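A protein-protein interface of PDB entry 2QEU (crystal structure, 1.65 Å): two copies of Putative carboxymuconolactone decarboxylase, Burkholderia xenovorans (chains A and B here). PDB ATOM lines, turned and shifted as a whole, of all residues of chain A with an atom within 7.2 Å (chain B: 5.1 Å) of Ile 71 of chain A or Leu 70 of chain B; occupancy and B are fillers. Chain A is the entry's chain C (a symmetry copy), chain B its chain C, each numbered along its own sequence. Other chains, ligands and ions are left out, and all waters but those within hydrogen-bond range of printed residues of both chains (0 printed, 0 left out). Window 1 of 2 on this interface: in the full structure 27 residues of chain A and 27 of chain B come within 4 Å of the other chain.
The side-chain hydroxyl of Tyr 67 of chain B lies within hydrogen-bond range of the side-chain carboxylate of Glu 101 of chain B, 2.6 Å away.
Among the printed residues, merely in contact across the chains: Tyr 67 of chain A with Tyr 67 of chain B (3.3 Å), Lys 68 of chain A with Leu 108 of chain B (3.3 Å), Leu 108 of chain A with Lys 68 of chain B (3.3 Å), Leu 63 of chain A with Tyr 67 of chain B (3.5 Å), Pro 64 of chain A with Tyr 67 of chain B (3.6 Å), Leu 63 of chain A with Gly 105 of chain B (3.7 Å), Leu 75 of chain A with Leu 108 of chain B (3.7 Å), Leu 108 of chain A with Leu 75 of chain B (3.7 Å), Leu 63 of chain A with Leu 70 of chain B (3.8 Å), Ile 71 of chain A with Leu 70 of chain B (3.8 Å), Leu 70 of chain A with Ile 71 of chain B (3.8 Å), Ile 71 of chain A with Gly 105 of chain B (3.8 Å), Pro 64 of chain A with Glu 101 of chain B (3.9 Å), Leu 72 of chain A with Leu 108 of chain B (3.9 Å), Leu 108 of chain A with Leu 72 of chain B (3.9 Å), Leu 75 of chain A with Val 74 of chain B (3.9 Å), Val 74 of chain A with Leu 75 of chain B (3.9 Å) and Leu 63 of chain A with Glu 101 of chain B (3.9 Å).
Printed residues of chain B within 4 Å of Ile 71 of chain A: Leu 70 (3.8 Å) and Gly 105 (3.8 Å).
Leu 70 of chain B touches two residues of chain A.
Printed residues of chain A within 4 Å of Leu 72 of chain B: Leu 108.
Of the printed residues of chain A, Tyr 67 of chain B touches Leu 63, Pro 64 and Tyr 67.
Of the printed residues of chain A, Gly 105 of chain B touches Leu 63 and Ile 71.
Printed residues of chain A within 4 Å of Lys 68 of chain B: Leu 108.
Ala 92 of chain B touches none of the printed residues of chain A.
Ile 106 of chain B touches none of the printed residues of chain A.
The nearest residue of chain A that does not touch Leu 70 of chain B is Tyr 67 of chain A (6.1 Å).
The nearest printed residue of chain B that does not touch Leu 108 of chain A is Ile 71 of chain B (4.1 Å).
Of the 18 printed residues of chain B, 10 touch a printed residue of chain A.
Hydrophobic or aromatic side chains of chain B within 4 Å of the printed part of chain A: Tyr 67, Leu 70, Ile 71, Leu 72, Val 74, Leu 75 and Leu 108.
Printed residues of chain A that touch a printed residue of chain B: Leu 63, Pro 64, Tyr 67, Lys 68, Leu 70, Ile 71, Leu 72, Val 74, Leu 75 and Leu 108.
Among the printed residues, no Asp or Glu carboxylate lies within 4 Å of a Lys or Arg side-chain nitrogen of the other chain.
Tyr 67 of chain B touches its own counterpart, Tyr 67 of chain A.
Lys 68 of chain A touches Leu 108 of chain B, and with the chains exchanged Leu 108 of chain A touches Lys 68 of chain B.
Val 74 of chain A touches Leu 75 of chain B, and with the chains exchanged Leu 75 of chain A touches Val 74 of chain B.
Leu 75 of chain A touches Leu 108 of chain B, and with the chains exchanged Leu 108 of chain A touches Leu 75 of chain B.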
ATOM      1  N   LEU A  63      -2.726   5.253  25.907  1.00  0.00           N
ATOM      2  CA  LEU A  63      -2.871   6.040  24.697  1.00  0.00           C
ATOM      3  C   LEU A  63      -2.915   7.529  25.130  1.00  0.00           C
ATOM      4  O   LEU A  63      -3.798   7.943  25.902  1.00  0.00           O
ATOM      5  CB  LEU A  63      -4.158   5.621  23.961  1.00  0.00           C
ATOM      6  CG  LEU A  63      -4.417   6.310  22.614  1.00  0.00           C
ATOM      7  CD1 LEU A  63      -3.246   6.021  21.635  1.00  0.00           C
ATOM      8  CD2 LEU A  63      -5.735   5.821  22.046  1.00  0.00           C
ATOM      9  N   PRO A  64      -1.990   8.344  24.621  1.00  0.00           N
ATOM     10  CA  PRO A  64      -2.018   9.746  24.937  1.00  0.00           C
ATOM     11  C   PRO A  64      -3.357  10.423  24.655  1.00  0.00           C
ATOM     12  O   PRO A  64      -4.026  10.152  23.644  1.00  0.00           O
ATOM     13  CB  PRO A  64      -0.888  10.336  24.080  1.00  0.00           C
ATOM     14  CG  PRO A  64       0.039   9.195  23.900  1.00  0.00           C
ATOM     15  CD  PRO A  64      -0.871   8.012  23.727  1.00  0.00           C
ATOM     16  N   LEU A  65      -3.705  11.310  25.586  1.00  0.00           N
ATOM     17  CA  LEU A  65      -4.990  11.979  25.537  1.00  0.00           C
ATOM     18  C   LEU A  65      -5.190  12.751  24.253  1.00  0.00           C
ATOM     19  O   LEU A  65      -6.296  12.792  23.696  1.00  0.00           O
ATOM     20  CB  LEU A  65      -5.140  12.922  26.732  1.00  0.00           C
ATOM     21  CG  LEU A  65      -6.546  13.516  26.926  1.00  0.00           C
ATOM     22  CD1 LEU A  65      -7.653  12.472  27.020  1.00  0.00           C
ATOM     23  CD2 LEU A  65      -6.510  14.492  28.169  1.00  0.00           C
ATOM     24  N   LYS A  66      -4.131  13.401  23.780  1.00  0.00           N
ATOM     25  CA  LYS A  66      -4.244  14.137  22.512  1.00  0.00           C
ATOM     26  C   LYS A  66      -4.677  13.192  21.363  1.00  0.00           C
ATOM     27  O   LYS A  66      -5.407  13.607  20.464  1.00  0.00           O
ATOM     28  CB  LYS A  66      -2.931  14.829  22.142  1.00  0.00           C
ATOM     29  CG  LYS A  66      -1.732  13.953  21.926  1.00  0.00           C
ATOM     30  CD  LYS A  66      -0.447  14.823  21.899  1.00  0.00           C
ATOM     31  CE  LYS A  66       0.807  14.003  21.776  1.00  0.00           C
ATOM     32  NZ  LYS A  66       2.021  14.909  21.748  1.00  0.00           N
ATOM     33  N   TYR A  67      -4.216  11.947  21.402  1.00  0.00           N
ATOM     34  CA  TYR A  67      -4.571  10.993  20.344  1.00  0.00           C
ATOM     35  C   TYR A  67      -5.954  10.383  20.581  1.00  0.00           C
ATOM     36  O   TYR A  67      -6.645  10.052  19.629  1.00  0.00           O
ATOM     37  CB  TYR A  67      -3.476   9.936  20.133  1.00  0.00           C
ATOM     38  CG  TYR A  67      -2.150  10.576  19.680  1.00  0.00           C
ATOM     39  CD1 TYR A  67      -2.097  11.522  18.665  1.00  0.00           C
ATOM     40  CD2 TYR A  67      -0.965  10.246  20.311  1.00  0.00           C
ATOM     41  CE1 TYR A  67      -0.891  12.128  18.312  1.00  0.00           C
ATOM     42  CE2 TYR A  67       0.231  10.845  19.973  1.00  0.00           C
ATOM     43  CZ  TYR A  67       0.276  11.768  18.978  1.00  0.00           C
ATOM     44  OH  TYR A  67       1.483  12.398  18.647  1.00  0.00           O
ATOM     45  N   LYS A  68      -6.354  10.162  21.834  1.00  0.00           N
ATOM     46  CA  LYS A  68      -7.754   9.810  22.132  1.00  0.00           C
ATOM     47  C   LYS A  68      -8.705  10.830  21.529  1.00  0.00           C
ATOM     48  O   LYS A  68      -9.610  10.455  20.789  1.00  0.00           O
ATOM     49  CB  LYS A  68      -8.001   9.673  23.628  1.00  0.00           C
ATOM     50  CG  LYS A  68      -7.179   8.623  24.335  1.00  0.00           C
ATOM     51  CD  LYS A  68      -7.670   8.384  25.721  1.00  0.00           C
ATOM     52  CE  LYS A  68      -7.078   7.149  26.385  1.00  0.00           C
ATOM     53  NZ  LYS A  68      -7.648   6.881  27.764  1.00  0.00           N
ATOM     54  N   HIS A  69      -8.441  12.129  21.777  1.00  0.00           N
ATOM     55  CA  HIS A  69      -9.305  13.192  21.211  1.00  0.00           C
ATOM     56  C   HIS A  69      -9.194  13.277  19.679  1.00  0.00           C
ATOM     57  O   HIS A  69     -10.174  13.510  19.018  1.00  0.00           O
ATOM     58  CB  HIS A  69      -9.113  14.521  21.914  1.00  0.00           C
ATOM     59  CG  HIS A  69      -9.800  14.572  23.243  1.00  0.00           C
ATOM     60  ND1 HIS A  69     -11.173  14.628  23.351  1.00  0.00           N
ATOM     61  CD2 HIS A  69      -9.317  14.450  24.500  1.00  0.00           C
ATOM     62  CE1 HIS A  69     -11.496  14.637  24.645  1.00  0.00           C
ATOM     63  NE2 HIS A  69     -10.391  14.529  25.371  1.00  0.00           N
ATOM     64  N   LEU A  70      -8.025  12.999  19.114  1.00  0.00           N
ATOM     65  CA  LEU A  70      -7.871  12.941  17.643  1.00  0.00           C
ATOM     66  C   LEU A  70      -8.744  11.838  17.005  1.00  0.00           C
ATOM     67  O   LEU A  70      -9.416  12.070  16.029  1.00  0.00           O
ATOM     68  CB  LEU A  70      -6.421  12.790  17.234  1.00  0.00           C
ATOM     69  CG  LEU A  70      -6.152  12.677  15.715  1.00  0.00           C
ATOM     70  CD1 LEU A  70      -6.724  13.896  14.965  1.00  0.00           C
ATOM     71  CD2 LEU A  70      -4.649  12.504  15.407  1.00  0.00           C
ATOM     72  N   ILE A  71      -8.797  10.685  17.638  1.00  0.00           N
ATOM     73  CA  ILE A  71      -9.665   9.607  17.193  1.00  0.00           C
ATOM     74  C   ILE A  71     -11.113  10.084  17.211  1.00  0.00           C
ATOM     75  O   ILE A  71     -11.876   9.879  16.272  1.00  0.00           O
ATOM     76  CB  ILE A  71      -9.474   8.305  18.009  1.00  0.00           C
ATOM     77  CG1 ILE A  71      -8.085   7.718  17.661  1.00  0.00           C
ATOM     78  CG2 ILE A  71     -10.639   7.305  17.753  1.00  0.00           C
ATOM     79  CD1 ILE A  71      -7.607   6.641  18.683  1.00  0.00           C
ATOM     80  N   LEU A  72     -11.541  10.774  18.262  1.00  0.00           N
ATOM     81  CA  LEU A  72     -12.897  11.264  18.332  1.00  0.00           C
ATOM     82  C   LEU A  72     -13.181  12.387  17.322  1.00  0.00           C
ATOM     83  O   LEU A  72     -14.303  12.502  16.828  1.00  0.00           O
ATOM     84  CB  LEU A  72     -13.163  11.690  19.784  1.00  0.00           C
ATOM     85  CG  LEU A  72     -13.371  10.518  20.785  1.00  0.00           C
ATOM     86  CD1 LEU A  72     -13.221  10.990  22.269  1.00  0.00           C
ATOM     87  CD2 LEU A  72     -14.787   9.922  20.530  1.00  0.00           C
ATOM     88  N   VAL A  73     -12.176  13.232  17.033  1.00  0.00           N
ATOM     89  CA  VAL A  73     -12.280  14.193  15.927  1.00  0.00           C
ATOM     90  C   VAL A  73     -12.624  13.457  14.619  1.00  0.00           C
ATOM     91  O   VAL A  73     -13.554  13.819  13.928  1.00  0.00           O
ATOM     92  CB  VAL A  73     -10.989  15.010  15.764  1.00  0.00           C
ATOM     93  CG1 VAL A  73     -11.003  15.747  14.386  1.00  0.00           C
ATOM     94  CG2 VAL A  73     -10.754  16.009  16.982  1.00  0.00           C
ATOM     95  N   VAL A  74     -11.869  12.426  14.294  1.00  0.00           N
ATOM     96  CA  VAL A  74     -12.077  11.711  13.049  1.00  0.00           C
ATOM     97  C   VAL A  74     -13.461  11.063  13.059  1.00  0.00           C
ATOM     98  O   VAL A  74     -14.200  11.069  12.071  1.00  0.00           O
ATOM     99  CB  VAL A  74     -10.923  10.718  12.777  1.00  0.00           C
ATOM    100  CG1 VAL A  74     -11.182   9.956  11.465  1.00  0.00           C
ATOM    101  CG2 VAL A  74      -9.590  11.415  12.665  1.00  0.00           C
ATOM    102  N   LEU A  75     -13.813  10.446  14.187  1.00  0.00           N
ATOM    103  CA  LEU A  75     -15.166   9.827  14.271  1.00  0.00           C
ATOM    104  C   LEU A  75     -16.276  10.874  14.108  1.00  0.00           C
ATOM    105  O   LEU A  75     -17.273  10.611  13.425  1.00  0.00           O
ATOM    106  CB  LEU A  75     -15.335   9.141  15.607  1.00  0.00           C
ATOM    107  CG  LEU A  75     -14.502   7.859  15.810  1.00  0.00           C
ATOM    108  CD1 LEU A  75     -14.543   7.372  17.253  1.00  0.00           C
ATOM    109  CD2 LEU A  75     -15.018   6.777  14.886  1.00  0.00           C
ATOM    110  N   ASP A  76     -16.111  12.049  14.711  1.00  0.00           N
ATOM    111  CA  ASP A  76     -17.096  13.124  14.567  1.00  0.00           C
ATOM    112  C   ASP A  76     -17.123  13.673  13.120  1.00  0.00           C
ATOM    113  O   ASP A  76     -18.188  14.118  12.630  1.00  0.00           O
ATOM    114  CB  ASP A  76     -16.873  14.233  15.577  1.00  0.00           C
ATOM    115  CG  ASP A  76     -17.366  13.876  16.981  1.00  0.00           C
ATOM    116  OD1 ASP A  76     -18.033  12.828  17.136  1.00  0.00           O
ATOM    117  OD2 ASP A  76     -17.094  14.751  17.852  1.00  0.00           O
ATOM    118  N   ALA A  77     -15.999  13.595  12.388  1.00  0.00           N
ATOM    119  CA  ALA A  77     -15.974  13.947  10.981  1.00  0.00           C
ATOM    120  C   ALA A  77     -16.870  12.992  10.191  1.00  0.00           C
ATOM    121  O   ALA A  77     -17.686  13.400   9.392  1.00  0.00           O
ATOM    122  CB  ALA A  77     -14.483  13.911  10.461  1.00  0.00           C
ATOM    123  N   HIS A  88     -13.713  18.375  20.416  1.00  0.00           N
ATOM    124  CA  HIS A  88     -12.650  17.382  20.481  1.00  0.00           C
ATOM    125  C   HIS A  88     -11.315  17.898  19.907  1.00  0.00           C
ATOM    126  O   HIS A  88     -10.270  17.514  20.357  1.00  0.00           O
ATOM    127  CB  HIS A  88     -13.082  16.071  19.862  1.00  0.00           C
ATOM    128  CG  HIS A  88     -14.004  15.303  20.750  1.00  0.00           C
ATOM    129  ND1 HIS A  88     -13.584  14.729  21.929  1.00  0.00           N
ATOM    130  CD2 HIS A  88     -15.331  15.082  20.664  1.00  0.00           C
ATOM    131  CE1 HIS A  88     -14.626  14.160  22.508  1.00  0.00           C
ATOM    132  NE2 HIS A  88     -15.703  14.363  21.769  1.00  0.00           N
ATOM    133  N   ALA A  92      -8.019  18.059  22.035  1.00  0.00           N
ATOM    134  CA  ALA A  92      -6.817  17.427  21.548  1.00  0.00           C
ATOM    135  C   ALA A  92      -5.634  18.402  21.589  1.00  0.00           C
ATOM    136  O   ALA A  92      -4.513  18.048  21.971  1.00  0.00           O
ATOM    137  CB  ALA A  92      -7.042  16.879  20.109  1.00  0.00           C
ATOM    138  N   LEU A 108      -7.106  10.743   6.841  1.00  0.00           N
ATOM    139  CA  LEU A 108      -7.252   9.290   6.769  1.00  0.00           C
ATOM    140  C   LEU A 108      -8.701   8.858   6.640  1.00  0.00           C
ATOM    141  O   LEU A 108      -9.023   7.786   6.093  1.00  0.00           O
ATOM    142  CB  LEU A 108      -6.639   8.645   8.019  1.00  0.00           C
ATOM    143  CG  LEU A 108      -5.126   8.884   8.191  1.00  0.00           C
ATOM    144  CD1 LEU A 108      -4.550   8.283   9.527  1.00  0.00           C
ATOM    145  CD2 LEU A 108      -4.350   8.314   6.955  1.00  0.00           C
ATOM    146  N   LEU B  65       3.252   6.963  12.750  1.00  0.00           N
ATOM    147  CA  LEU B  65       2.657   5.955  11.895  1.00  0.00           C
ATOM    148  C   LEU B  65       1.784   4.989  12.663  1.00  0.00           C
ATOM    149  O   LEU B  65       0.727   4.559  12.180  1.00  0.00           O
ATOM    150  CB  LEU B  65       3.748   5.181  11.152  1.00  0.00           C
ATOM    151  CG  LEU B  65       3.246   4.244  10.042  1.00  0.00           C
ATOM    152  CD1 LEU B  65       2.375   4.931   8.996  1.00  0.00           C
ATOM    153  CD2 LEU B  65       4.491   3.499   9.415  1.00  0.00           C
ATOM    154  N   LYS B  66       2.226   4.610  13.858  1.00  0.00           N
ATOM    155  CA  LYS B  66       1.405   3.706  14.677  1.00  0.00           C
ATOM    156  C   LYS B  66       0.009   4.321  14.946  1.00  0.00           C
ATOM    157  O   LYS B  66      -0.983   3.596  15.018  1.00  0.00           O
ATOM    158  CB  LYS B  66       2.086   3.374  16.006  1.00  0.00           C
ATOM    159  CG  LYS B  66       2.369   4.516  16.935  1.00  0.00           C
ATOM    160  CD  LYS B  66       3.346   4.054  18.050  1.00  0.00           C
ATOM    161  CE  LYS B  66       3.748   5.173  18.969  1.00  0.00           C
ATOM    162  NZ  LYS B  66       4.693   4.656  20.036  1.00  0.00           N
ATOM    163  N   TYR B  67      -0.048   5.639  15.101  1.00  0.00           N
ATOM    164  CA  TYR B  67      -1.333   6.297  15.371  1.00  0.00           C
ATOM    165  C   TYR B  67      -2.133   6.513  14.084  1.00  0.00           C
ATOM    166  O   TYR B  67      -3.354   6.500  14.117  1.00  0.00           O
ATOM    167  CB  TYR B  67      -1.157   7.583  16.193  1.00  0.00           C
ATOM    168  CG  TYR B  67      -0.547   7.293  17.578  1.00  0.00           C
ATOM    169  CD1 TYR B  67      -1.019   6.271  18.391  1.00  0.00           C
ATOM    170  CD2 TYR B  67       0.530   8.030  18.034  1.00  0.00           C
ATOM    171  CE1 TYR B  67      -0.412   5.992  19.615  1.00  0.00           C
ATOM    172  CE2 TYR B  67       1.140   7.756  19.240  1.00  0.00           C
ATOM    173  CZ  TYR B  67       0.673   6.757  20.032  1.00  0.00           C
ATOM    174  OH  TYR B  67       1.303   6.459  21.248  1.00  0.00           O
ATOM    175  N   LYS B  68      -1.475   6.780  12.955  1.00  0.00           N
ATOM    176  CA  LYS B  68      -2.164   6.756  11.653  1.00  0.00           C
ATOM    177  C   LYS B  68      -2.885   5.434  11.451  1.00  0.00           C
ATOM    178  O   LYS B  68      -4.083   5.430  11.180  1.00  0.00           O
ATOM    179  CB  LYS B  68      -1.209   7.021  10.498  1.00  0.00           C
ATOM    180  CG  LYS B  68      -0.490   8.349  10.531  1.00  0.00           C
ATOM    181  CD  LYS B  68       0.210   8.626   9.245  1.00  0.00           C
ATOM    182  CE  LYS B  68       0.708  10.057   9.106  1.00  0.00           C
ATOM    183  NZ  LYS B  68       1.349  10.338   7.761  1.00  0.00           N
ATOM    184  N   HIS B  69      -2.172   4.312  11.673  1.00  0.00           N
ATOM    185  CA  HIS B  69      -2.803   2.979  11.520  1.00  0.00           C
ATOM    186  C   HIS B  69      -3.880   2.720  12.587  1.00  0.00           C
ATOM    187  O   HIS B  69      -4.887   2.129  12.293  1.00  0.00           O
ATOM    188  CB  HIS B  69      -1.777   1.870  11.403  1.00  0.00           C
ATOM    189  CG  HIS B  69      -1.151   1.808  10.045  1.00  0.00           C
ATOM    190  ND1 HIS B  69      -1.853   1.378   8.939  1.00  0.00           N
ATOM    191  CD2 HIS B  69       0.052   2.234   9.599  1.00  0.00           C
ATOM    192  CE1 HIS B  69      -1.053   1.455   7.874  1.00  0.00           C
ATOM    193  NE2 HIS B  69       0.112   1.972   8.240  1.00  0.00           N
ATOM    194  N   LEU B  70      -3.709   3.240  13.797  1.00  0.00           N
ATOM    195  CA  LEU B  70      -4.755   3.137  14.840  1.00  0.00           C
ATOM    196  C   LEU B  70      -6.064   3.847  14.428  1.00  0.00           C
ATOM    197  O   LEU B  70      -7.132   3.300  14.567  1.00  0.00           O
ATOM    198  CB  LEU B  70      -4.265   3.638  16.181  1.00  0.00           C
ATOM    199  CG  LEU B  70      -5.296   3.613  17.334  1.00  0.00           C
ATOM    200  CD1 LEU B  70      -5.852   2.191  17.541  1.00  0.00           C
ATOM    201  CD2 LEU B  70      -4.705   4.164  18.649  1.00  0.00           C
ATOM    202  N   ILE B  71      -5.942   5.012  13.828  1.00  0.00           N
ATOM    203  CA  ILE B  71      -7.093   5.726  13.302  1.00  0.00           C
ATOM    204  C   ILE B  71      -7.788   4.863  12.254  1.00  0.00           C
ATOM    205  O   ILE B  71      -9.005   4.710  12.241  1.00  0.00           O
ATOM    206  CB  ILE B  71      -6.733   7.128  12.751  1.00  0.00           C
ATOM    207  CG1 ILE B  71      -6.356   8.033  13.948  1.00  0.00           C
ATOM    208  CG2 ILE B  71      -7.892   7.709  11.890  1.00  0.00           C
ATOM    209  CD1 ILE B  71      -5.607   9.331  13.516  1.00  0.00           C
ATOM    210  N   LEU B  72      -7.040   4.230  11.356  1.00  0.00           N
ATOM    211  CA  LEU B  72      -7.637   3.389  10.347  1.00  0.00           C
ATOM    212  C   LEU B  72      -8.250   2.103  10.925  1.00  0.00           C
ATOM    213  O   LEU B  72      -9.248   1.606  10.401  1.00  0.00           O
ATOM    214  CB  LEU B  72      -6.565   3.107   9.283  1.00  0.00           C
ATOM    215  CG  LEU B  72      -6.259   4.297   8.329  1.00  0.00           C
ATOM    216  CD1 LEU B  72      -4.907   4.096   7.567  1.00  0.00           C
ATOM    217  CD2 LEU B  72      -7.448   4.424   7.331  1.00  0.00           C
ATOM    218  N   VAL B  73      -7.644   1.549  11.990  1.00  0.00           N
ATOM    219  CA  VAL B  73      -8.273   0.456  12.743  1.00  0.00           C
ATOM    220  C   VAL B  73      -9.678   0.876  13.210  1.00  0.00           C
ATOM    221  O   VAL B  73     -10.642   0.173  12.989  1.00  0.00           O
ATOM    222  CB  VAL B  73      -7.411   0.027  13.941  1.00  0.00           C
ATOM    223  CG1 VAL B  73      -8.258  -0.865  14.905  1.00  0.00           C
ATOM    224  CG2 VAL B  73      -6.062  -0.686  13.485  1.00  0.00           C
ATOM    225  N   VAL B  74      -9.780   2.026  13.849  1.00  0.00           N
ATOM    226  CA  VAL B  74     -11.052   2.473  14.382  1.00  0.00           C
ATOM    227  C   VAL B  74     -12.036   2.695  13.233  1.00  0.00           C
ATOM    228  O   VAL B  74     -13.217   2.343  13.299  1.00  0.00           O
ATOM    229  CB  VAL B  74     -10.870   3.707  15.296  1.00  0.00           C
ATOM    230  CG1 VAL B  74     -12.237   4.176  15.827  1.00  0.00           C
ATOM    231  CG2 VAL B  74      -9.981   3.411  16.477  1.00  0.00           C
ATOM    232  N   LEU B  75     -11.558   3.334  12.166  1.00  0.00           N
ATOM    233  CA  LEU B  75     -12.459   3.546  10.998  1.00  0.00           C
ATOM    234  C   LEU B  75     -12.932   2.215  10.400  1.00  0.00           C
ATOM    235  O   LEU B  75     -14.107   2.086  10.038  1.00  0.00           O
ATOM    236  CB  LEU B  75     -11.737   4.333   9.928  1.00  0.00           C
ATOM    237  CG  LEU B  75     -11.463   5.814  10.257  1.00  0.00           C
ATOM    238  CD1 LEU B  75     -10.527   6.462   9.245  1.00  0.00           C
ATOM    239  CD2 LEU B  75     -12.776   6.566  10.302  1.00  0.00           C
ATOM    240  N   ALA B  92      -0.038  -1.157  12.644  1.00  0.00           N
ATOM    241  CA  ALA B  92       0.111  -0.281  13.781  1.00  0.00           C
ATOM    242  C   ALA B  92       1.109  -0.864  14.789  1.00  0.00           C
ATOM    243  O   ALA B  92       1.952  -0.155  15.352  1.00  0.00           O
ATOM    244  CB  ALA B  92      -1.271  -0.024  14.448  1.00  0.00           C
ATOM    245  N   LEU B  97       2.785   0.335  18.119  1.00  0.00           N
ATOM    246  CA  LEU B  97       1.541   0.445  18.909  1.00  0.00           C
ATOM    247  C   LEU B  97       1.475  -0.749  19.893  1.00  0.00           C
ATOM    248  O   LEU B  97       1.688  -1.880  19.487  1.00  0.00           O
ATOM    249  CB  LEU B  97       0.293   0.409  18.019  1.00  0.00           C
ATOM    250  CG  LEU B  97      -0.964   0.919  18.730  1.00  0.00           C
ATOM    251  CD1 LEU B  97      -0.935   2.483  18.862  1.00  0.00           C
ATOM    252  CD2 LEU B  97      -2.293   0.436  18.080  1.00  0.00           C
ATOM    253  N   GLU B 101      -2.865   0.321  23.952  1.00  0.00           N
ATOM    254  CA  GLU B 101      -3.231   1.478  23.124  1.00  0.00           C
ATOM    255  C   GLU B 101      -4.305   1.122  22.115  1.00  0.00           C
ATOM    256  O   GLU B 101      -5.237   1.911  21.881  1.00  0.00           O
ATOM    257  CB  GLU B 101      -2.030   2.046  22.418  1.00  0.00           C
ATOM    258  CG  GLU B 101      -1.035   2.701  23.339  1.00  0.00           C
ATOM    259  CD  GLU B 101       0.105   3.252  22.544  1.00  0.00           C
ATOM    260  OE1 GLU B 101       0.782   2.484  21.795  1.00  0.00           O
ATOM    261  OE2 GLU B 101       0.307   4.466  22.629  1.00  0.00           O
ATOM    262  N   LEU B 102      -4.167  -0.038  21.481  1.00  0.00           N
ATOM    263  CA  LEU B 102      -5.141  -0.493  20.515  1.00  0.00           C
ATOM    264  C   LEU B 102      -6.515  -0.572  21.160  1.00  0.00           C
ATOM    265  O   LEU B 102      -7.523  -0.041  20.623  1.00  0.00           O
ATOM    266  CB  LEU B 102      -4.747  -1.864  19.952  1.00  0.00           C
ATOM    267  CG  LEU B 102      -5.683  -2.485  18.919  1.00  0.00           C
ATOM    268  CD1 LEU B 102      -5.507  -1.827  17.569  1.00  0.00           C
ATOM    269  CD2 LEU B 102      -5.437  -3.995  18.832  1.00  0.00           C
ATOM    270  N   GLY B 105      -8.027   2.920  22.036  1.00  0.00           N
ATOM    271  CA  GLY B 105      -8.529   3.623  20.872  1.00  0.00           C
ATOM    272  C   GLY B 105      -9.829   3.043  20.299  1.00  0.00           C
ATOM    273  O   GLY B 105     -10.737   3.775  19.984  1.00  0.00           O
ATOM    274  N   ILE B 106      -9.898   1.706  20.139  1.00  0.00           N
ATOM    275  CA  ILE B 106     -11.099   1.053  19.592  1.00  0.00           C
ATOM    276  C   ILE B 106     -12.315   1.365  20.472  1.00  0.00           C
ATOM    277  O   ILE B 106     -13.444   1.569  20.000  1.00  0.00           O
ATOM    278  CB  ILE B 106     -10.886  -0.464  19.392  1.00  0.00           C
ATOM    279  CG1 ILE B 106      -9.862  -0.770  18.286  1.00  0.00           C
ATOM    280  CG2 ILE B 106     -12.217  -1.198  19.118  1.00  0.00           C
ATOM    281  CD1 ILE B 106      -9.410  -2.274  18.268  1.00  0.00           C
ATOM    282  N   LEU B 108     -13.157   3.958  21.968  1.00  0.00           N
ATOM    283  CA  LEU B 108     -13.712   5.284  21.703  1.00  0.00           C
ATOM    284  C   LEU B 108     -14.778   5.263  20.623  1.00  0.00           C
ATOM    285  O   LEU B 108     -15.687   6.114  20.577  1.00  0.00           O
ATOM    286  CB  LEU B 108     -12.588   6.242  21.289  1.00  0.00           C
ATOM    287  CG  LEU B 108     -11.508   6.471  22.364  1.00  0.00           C
ATOM    288  CD1 LEU B 108     -10.326   7.389  21.873  1.00  0.00           C
ATOM    289  CD2 LEU B 108     -12.159   7.064  23.660  1.00  0.00           C
